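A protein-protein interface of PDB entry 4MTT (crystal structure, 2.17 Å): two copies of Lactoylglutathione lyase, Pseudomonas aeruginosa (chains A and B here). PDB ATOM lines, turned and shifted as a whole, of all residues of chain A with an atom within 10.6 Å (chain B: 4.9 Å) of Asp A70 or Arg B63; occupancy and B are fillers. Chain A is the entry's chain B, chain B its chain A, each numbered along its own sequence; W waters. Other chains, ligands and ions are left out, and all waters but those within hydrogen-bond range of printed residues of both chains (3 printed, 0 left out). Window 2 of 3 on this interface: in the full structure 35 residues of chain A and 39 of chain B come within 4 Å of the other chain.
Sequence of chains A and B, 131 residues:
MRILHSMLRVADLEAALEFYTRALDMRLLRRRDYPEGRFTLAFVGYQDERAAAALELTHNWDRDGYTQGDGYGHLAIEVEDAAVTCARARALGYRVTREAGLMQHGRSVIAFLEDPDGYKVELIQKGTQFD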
ATOM      1  N   THR A  67       9.868  -4.654   6.342  1.00  0.00           N
ATOM      2  CA  THR A  67       8.651  -4.452   7.118  1.00  0.00           C
ATOM      3  C   THR A  67       9.120  -4.358   8.570  1.00  0.00           C
ATOM      4  O   THR A  67       9.582  -5.354   9.122  1.00  0.00           O
ATOM      5  CB  THR A  67       7.675  -5.630   6.928  1.00  0.00           C
ATOM      6  OG1 THR A  67       7.360  -5.779   5.539  1.00  0.00           O
ATOM      7  CG2 THR A  67       6.388  -5.453   7.745  1.00  0.00           C
ATOM      8  N   GLN A  68       9.013  -3.177   9.173  1.00  0.00           N
ATOM      9  CA  GLN A  68       9.426  -2.963  10.552  1.00  0.00           C
ATOM     10  C   GLN A  68       8.322  -3.386  11.505  1.00  0.00           C
ATOM     11  O   GLN A  68       7.175  -2.942  11.373  1.00  0.00           O
ATOM     12  CB  GLN A  68       9.759  -1.471  10.796  1.00  0.00           C
ATOM     13  CG  GLN A  68      11.224  -1.132  10.506  1.00  0.00           C
ATOM     14  CD  GLN A  68      11.616   0.316  10.771  1.00  0.00           C
ATOM     15  OE1 GLN A  68      11.022   1.050  11.573  1.00  0.00           O
ATOM     16  NE2 GLN A  68      12.681   0.738  10.141  1.00  0.00           N
ATOM     17  N   GLY A  69       8.691  -4.189  12.497  1.00  0.00           N
ATOM     18  CA  GLY A  69       7.761  -4.603  13.547  1.00  0.00           C
ATOM     19  C   GLY A  69       7.711  -3.513  14.595  1.00  0.00           C
ATOM     20  O   GLY A  69       8.343  -2.464  14.426  1.00  0.00           O
ATOM     21  N   ASP A  70       6.994  -3.753  15.704  1.00  0.00           N
ATOM     22  CA  ASP A  70       6.896  -2.754  16.756  1.00  0.00           C
ATOM     23  C   ASP A  70       7.684  -3.144  18.027  1.00  0.00           C
ATOM     24  O   ASP A  70       7.534  -2.496  19.067  1.00  0.00           O
ATOM     25  CB  ASP A  70       5.404  -2.484  17.075  1.00  0.00           C
ATOM     26  CG  ASP A  70       4.577  -3.730  17.389  1.00  0.00           C
ATOM     27  OD1 ASP A  70       5.158  -4.730  17.853  1.00  0.00           O
ATOM     28  OD2 ASP A  70       3.358  -3.709  17.136  1.00  0.00           O
ATOM     29  N   GLY A  71       8.464  -4.221  17.944  1.00  0.00           N
ATOM     30  CA  GLY A  71       9.253  -4.697  19.069  1.00  0.00           C
ATOM     31  C   GLY A  71      10.564  -3.927  19.195  1.00  0.00           C
ATOM     32  O   GLY A  71      10.907  -3.448  20.282  1.00  0.00           O
ATOM     33  N   TYR A  72      11.298  -3.786  18.075  1.00  0.00           N
ATOM     34  CA  TYR A  72      12.581  -3.087  18.082  1.00  0.00           C
ATOM     35  C   TYR A  72      12.471  -1.651  18.555  1.00  0.00           C
ATOM     36  O   TYR A  72      11.612  -0.898  18.085  1.00  0.00           O
ATOM     37  CB  TYR A  72      13.323  -3.207  16.738  1.00  0.00           C
ATOM     38  CG  TYR A  72      14.622  -2.436  16.759  1.00  0.00           C
ATOM     39  CD1 TYR A  72      15.672  -2.833  17.583  1.00  0.00           C
ATOM     40  CD2 TYR A  72      14.767  -1.248  16.042  1.00  0.00           C
ATOM     41  CE1 TYR A  72      16.847  -2.100  17.664  1.00  0.00           C
ATOM     42  CE2 TYR A  72      15.952  -0.498  16.121  1.00  0.00           C
ATOM     43  CZ  TYR A  72      16.984  -0.934  16.940  1.00  0.00           C
ATOM     44  OH  TYR A  72      18.170  -0.263  17.051  1.00  0.00           O
ATOM     45  N   GLY A  73      13.318  -1.298  19.514  1.00  0.00           N
ATOM     46  CA  GLY A  73      13.293   0.035  20.090  1.00  0.00           C
ATOM     47  C   GLY A  73      14.166   1.079  19.428  1.00  0.00           C
ATOM     48  O   GLY A  73      13.684   1.923  18.661  1.00  0.00           O
ATOM     49  N   HIS A  74      15.450   1.081  19.802  1.00  0.00           N
ATOM     50  CA  HIS A  74      16.413   2.077  19.335  1.00  0.00           C
ATOM     51  C   HIS A  74      17.842   1.659  19.715  1.00  0.00           C
ATOM     52  O   HIS A  74      18.046   0.677  20.431  1.00  0.00           O
ATOM     53  CB  HIS A  74      16.082   3.462  19.974  1.00  0.00           C
ATOM     54  CG  HIS A  74      16.031   3.450  21.486  1.00  0.00           C
ATOM     55  ND1 HIS A  74      14.823   3.578  22.180  1.00  0.00           N
ATOM     56  CD2 HIS A  74      17.044   3.382  22.386  1.00  0.00           C
ATOM     57  CE1 HIS A  74      15.142   3.585  23.464  1.00  0.00           C
ATOM     58  NE2 HIS A  74      16.468   3.443  23.640  1.00  0.00           N
ATOM     59  N   GLY A 118      14.269   4.559   8.904  1.00  0.00           N
ATOM     60  CA  GLY A 118      13.291   4.819   9.950  1.00  0.00           C
ATOM     61  C   GLY A 118      13.669   4.320  11.329  1.00  0.00           C
ATOM     62  O   GLY A 118      12.850   4.424  12.249  1.00  0.00           O
ATOM     63  N   TYR A 119      14.911   3.787  11.504  1.00  0.00           N
ATOM     64  CA  TYR A 119      15.365   3.311  12.813  1.00  0.00           C
ATOM     65  C   TYR A 119      15.693   4.493  13.683  1.00  0.00           C
ATOM     66  O   TYR A 119      16.229   5.483  13.191  1.00  0.00           O
ATOM     67  CB  TYR A 119      16.566   2.382  12.701  1.00  0.00           C
ATOM     68  CG  TYR A 119      16.334   1.131  11.878  1.00  0.00           C
ATOM     69  CD1 TYR A 119      15.383   0.185  12.259  1.00  0.00           C
ATOM     70  CD2 TYR A 119      17.098   0.872  10.740  1.00  0.00           C
ATOM     71  CE1 TYR A 119      15.233  -1.016  11.551  1.00  0.00           C
ATOM     72  CE2 TYR A 119      16.947  -0.310  10.018  1.00  0.00           C
ATOM     73  CZ  TYR A 119      15.993  -1.237  10.408  1.00  0.00           C
ATOM     74  OH  TYR A 119      15.824  -2.353   9.632  1.00  0.00           O
ATOM     75  N   LYS A 120      15.312   4.424  14.963  1.00  0.00           N
ATOM     76  CA  LYS A 120      15.526   5.516  15.925  1.00  0.00           C
ATOM     77  C   LYS A 120      16.873   5.422  16.597  1.00  0.00           C
ATOM     78  O   LYS A 120      17.306   4.330  16.968  1.00  0.00           O
ATOM     79  CB  LYS A 120      14.410   5.566  16.997  1.00  0.00           C
ATOM     80  CG  LYS A 120      13.007   5.821  16.427  1.00  0.00           C
ATOM     81  CD  LYS A 120      12.789   7.281  15.964  1.00  0.00           C
ATOM     82  CE  LYS A 120      11.316   7.641  15.837  1.00  0.00           C
ATOM     83  NZ  LYS A 120      11.113   8.927  15.113  1.00  0.00           N
ATOM     84  N   ARG B   9      11.704  -4.375  23.019  1.00  0.00           N
ATOM     85  CA  ARG B   9      10.476  -4.488  23.796  1.00  0.00           C
ATOM     86  C   ARG B   9      10.162  -5.968  23.998  1.00  0.00           C
ATOM     87  O   ARG B   9      10.246  -6.779  23.063  1.00  0.00           O
ATOM     88  CB  ARG B   9       9.303  -3.725  23.153  1.00  0.00           C
ATOM     89  CG  ARG B   9       9.468  -2.207  23.203  1.00  0.00           C
ATOM     90  CD  ARG B   9       8.338  -1.459  22.515  1.00  0.00           C
ATOM     91  NE  ARG B   9       8.741  -0.076  22.288  1.00  0.00           N
ATOM     92  CZ  ARG B   9       9.289   0.392  21.169  1.00  0.00           C
ATOM     93  NH1 ARG B   9       9.411  -0.387  20.101  1.00  0.00           N
ATOM     94  NH2 ARG B   9       9.690   1.652  21.101  1.00  0.00           N
ATOM     95  N   ALA B  11       7.438  -8.924  25.986  1.00  0.00           N
ATOM     96  CA  ALA B  11       6.064  -9.206  26.428  1.00  0.00           C
ATOM     97  C   ALA B  11       6.056  -9.604  27.910  1.00  0.00           C
ATOM     98  O   ALA B  11       5.123  -9.316  28.635  1.00  0.00           O
ATOM     99  CB  ALA B  11       5.494 -10.374  25.597  1.00  0.00           C
ATOM    100  N   ASN B  60       6.277  -2.921  28.918  1.00  0.00           N
ATOM    101  CA  ASN B  60       5.062  -2.135  29.092  1.00  0.00           C
ATOM    102  C   ASN B  60       4.044  -3.083  29.767  1.00  0.00           C
ATOM    103  O   ASN B  60       3.624  -4.076  29.167  1.00  0.00           O
ATOM    104  CB  ASN B  60       4.579  -1.585  27.750  1.00  0.00           C
ATOM    105  CG  ASN B  60       5.563  -0.627  27.109  1.00  0.00           C
ATOM    106  OD1 ASN B  60       6.077  -0.869  26.008  1.00  0.00           O
ATOM    107  ND2 ASN B  60       5.859   0.483  27.783  1.00  0.00           N
ATOM    108  N   TRP B  61       3.734  -2.816  31.061  1.00  0.00           N
ATOM    109  CA  TRP B  61       2.875  -3.635  31.916  1.00  0.00           C
ATOM    110  C   TRP B  61       1.531  -3.997  31.290  1.00  0.00           C
ATOM    111  O   TRP B  61       1.019  -5.077  31.561  1.00  0.00           O
ATOM    112  CB  TRP B  61       2.640  -2.952  33.274  1.00  0.00           C
ATOM    113  CG  TRP B  61       3.864  -2.624  34.099  1.00  0.00           C
ATOM    114  CD1 TRP B  61       5.173  -2.784  33.746  1.00  0.00           C
ATOM    115  CD2 TRP B  61       3.870  -1.947  35.364  1.00  0.00           C
ATOM    116  NE1 TRP B  61       5.993  -2.310  34.742  1.00  0.00           N
ATOM    117  CE2 TRP B  61       5.217  -1.816  35.763  1.00  0.00           C
ATOM    118  CE3 TRP B  61       2.856  -1.507  36.238  1.00  0.00           C
ATOM    119  CZ2 TRP B  61       5.584  -1.281  37.006  1.00  0.00           C
ATOM    120  CZ3 TRP B  61       3.217  -0.967  37.464  1.00  0.00           C
ATOM    121  CH2 TRP B  61       4.568  -0.862  37.839  1.00  0.00           C
ATOM    122  N   ASP B  62       0.981  -3.112  30.451  1.00  0.00           N
ATOM    123  CA  ASP B  62      -0.289  -3.345  29.795  1.00  0.00           C
ATOM    124  C   ASP B  62      -0.200  -3.841  28.329  1.00  0.00           C
ATOM    125  O   ASP B  62      -1.237  -4.029  27.719  1.00  0.00           O
ATOM    126  CB  ASP B  62      -1.240  -2.140  29.984  1.00  0.00           C
ATOM    127  CG  ASP B  62      -1.294  -1.664  31.433  1.00  0.00           C
ATOM    128  OD1 ASP B  62      -1.521  -2.504  32.327  1.00  0.00           O
ATOM    129  OD2 ASP B  62      -0.986  -0.484  31.681  1.00  0.00           O
ATOM    130  N   ARG B  63       1.008  -4.067  27.772  1.00  0.00           N
ATOM    131  CA  ARG B  63       1.174  -4.605  26.403  1.00  0.00           C
ATOM    132  C   ARG B  63       1.420  -6.094  26.560  1.00  0.00           C
ATOM    133  O   ARG B  63       2.426  -6.488  27.169  1.00  0.00           O
ATOM    134  CB  ARG B  63       2.383  -3.990  25.642  1.00  0.00           C
ATOM    135  CG  ARG B  63       2.167  -2.625  24.981  1.00  0.00           C
ATOM    136  CD  ARG B  63       1.193  -2.599  23.808  1.00  0.00           C
ATOM    137  NE  ARG B  63       1.608  -3.395  22.645  1.00  0.00           N
ATOM    138  CZ  ARG B  63       2.322  -2.925  21.625  1.00  0.00           C
ATOM    139  NH1 ARG B  63       2.779  -1.679  21.643  1.00  0.00           N
ATOM    140  NH2 ARG B  63       2.605  -3.707  20.591  1.00  0.00           N
ATOM    141  N   ASP B  64       0.518  -6.916  26.014  1.00  0.00           N
ATOM    142  CA  ASP B  64       0.620  -8.381  26.065  1.00  0.00           C
ATOM    143  C   ASP B  64       1.680  -8.901  25.118  1.00  0.00           C
ATOM    144  O   ASP B  64       2.235  -9.966  25.381  1.00  0.00           O
ATOM    145  CB  ASP B  64      -0.725  -9.038  25.680  1.00  0.00           C
ATOM    146  CG  ASP B  64      -1.628  -9.481  26.824  1.00  0.00           C
ATOM    147  OD1 ASP B  64      -1.293  -9.193  28.001  1.00  0.00           O
ATOM    148  OD2 ASP B  64      -2.716 -10.037  26.542  1.00  0.00           O
ATOM    149  N   GLY B  65       1.870  -8.215  23.984  1.00  0.00           N
ATOM    150  CA  GLY B  65       2.806  -8.633  22.949  1.00  0.00           C
ATOM    151  C   GLY B  65       3.165  -7.589  21.907  1.00  0.00           C
ATOM    152  O   GLY B  65       2.605  -6.496  21.869  1.00  0.00           O
ATOM    153  N   TYR B  66       4.142  -7.942  21.074  1.00  0.00           N
ATOM    154  CA  TYR B  66       4.729  -7.118  20.018  1.00  0.00           C
ATOM    155  C   TYR B  66       4.741  -7.871  18.691  1.00  0.00           C
ATOM    156  O   TYR B  66       4.741  -9.100  18.678  1.00  0.00           O
ATOM    157  CB  TYR B  66       6.174  -6.693  20.419  1.00  0.00           C
ATOM    158  CG  TYR B  66       6.145  -5.817  21.647  1.00  0.00           C
ATOM    159  CD1 TYR B  66       6.341  -6.363  22.921  1.00  0.00           C
ATOM    160  CD2 TYR B  66       5.724  -4.490  21.568  1.00  0.00           C
ATOM    161  CE1 TYR B  66       6.171  -5.591  24.074  1.00  0.00           C
ATOM    162  CE2 TYR B  66       5.544  -3.714  22.711  1.00  0.00           C
ATOM    163  CZ  TYR B  66       5.788  -4.261  23.960  1.00  0.00           C
ATOM    164  OH  TYR B  66       5.664  -3.469  25.076  1.00  0.00           O
ATOM    165  N   THR B  67       4.698  -7.132  17.575  1.00  0.00           N
ATOM    166  CA  THR B  67       4.804  -7.747  16.269  1.00  0.00           C
ATOM    167  C   THR B  67       6.250  -7.657  15.790  1.00  0.00           C
ATOM    168  O   THR B  67       6.851  -6.592  15.815  1.00  0.00           O
ATOM    169  CB  THR B  67       3.742  -7.209  15.319  1.00  0.00           C
ATOM    170  OG1 THR B  67       2.468  -7.522  15.858  1.00  0.00           O
ATOM    171  CG2 THR B  67       3.828  -7.810  13.937  1.00  0.00           C
HETATM  172  O   HOH W   1       1.849  -5.476  17.765  1.00  0.00           O
HETATM  173  O   HOH W   2       6.106  -0.148  19.671  1.00  0.00           O
HETATM  174  O   HOH W   3      11.063   2.323  18.707  1.00  0.00           O
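The guanidinium group of Arg B9 is in hydrogen-bond range of the backbone carbonyl oxygen of Asp A70 (3.0 Å). The backbone carbonyl oxygen of Gly A71 lies within hydrogen-bond range of the backbone NH of Arg B9, 3.0 Å away. The backbone carbonyl oxygen (O) of Tyr A72 lies within hydrogen-bond range of the guanidinium group (NH1) of Arg B9, at 3.0 Å. The side-chain carboxylate of Asp A70 is in salt-bridge range of the guanidinium group of Arg B63. OD1 of Asp A70 sits at hydrogen-bond distance from N of Thr B67, 2.5 Å away.
The side-chain amide oxygen of Asn B60 lies within hydrogen-bond range of the side-chain hydroxyl of Tyr B66 (2.8 Å). NH2 of Arg B63 lies within hydrogen-bond range of O of Gly B65 (3.1 Å).
Gly A69 touches Thr B67. Asp A70 touches Tyr B66. CB of Tyr B66 touches CA of Gly A71 (3.9 Å). N of Gly A71 touches O of Thr B67, 3.6 Å away. Arg B9 touches Gly A73 (NH1 to CA, 3.9 Å).
Of the printed residues of chain B, Gly A69 touches Thr B67. Asp A70 touches just these residues of chain B: Arg B9, Arg B63, Tyr B66 and Thr B67. Printed residues of chain B within 4 Å of Gly A71: Arg B9, Tyr B66 and Thr B67. Printed residues of chain B within 4 Å of Tyr A72: Arg B9. Of the printed residues of chain B, Gly A73 touches Arg B9. His A74 touches none of the printed residues of chain B. Gly A118 touches none of the printed residues of chain B. Of the printed residues of chain A, Arg B9 touches Asp A70 (3.0 Å), Gly A71 (3.0 Å), Tyr A72 (3.0 Å) and Gly A73 (3.9 Å). No residue of chain A comes within 4 Å of Asn B60. No residue of chain A comes within 4 Å of Asp B62. Of chain A, only Asp A70 (3.5 Å) comes within 4 Å of Arg B63. Asp B64 touches none of the printed residues of chain A. No residue of chain A comes within 4 Å of Gly B65. Thr B67 touches three residues of chain A.
Of the 11 printed residues of chain A, 5 touch a printed residue of chain B. Printed residues of chain A that touch a printed residue of chain B: Gly A69, Asp A70, Gly A71, Tyr A72 and Gly A73. Of the 10 printed residues of chain B, 4 touch a printed residue of chain A. Hydrophobic or aromatic side chains of chain B within 4 Å of the printed part of chain A: Tyr B66. Among the printed residues, 10 pairs touch across the chains. Among the printed residues, Asp or Glu carboxylates within 4 Å of a Lys or Arg side-chain nitrogen of the other chain: Asp A70 with Arg B63 (3.5 Å).
Position printed for both chains: 67. Of the 10 pairs that touch across the chains among the printed residues, none has its exchanged pair printed and touching as well.
Water W1 lies within hydrogen-bond range of the side-chain carboxylate of Asp A70, the side-chain hydroxyl of Thr B67 and the guanidinium group of Arg B63. Water W3 lies within hydrogen-bond range of O of Gly A73, NH2 of Arg B9 and O of Tyr A72. Water W2 bridges the backbone carbonyl oxygen (O) of Asp A70 (2.8 Å) and the guanidinium group (NH1) of Arg B9 (3.3 Å).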
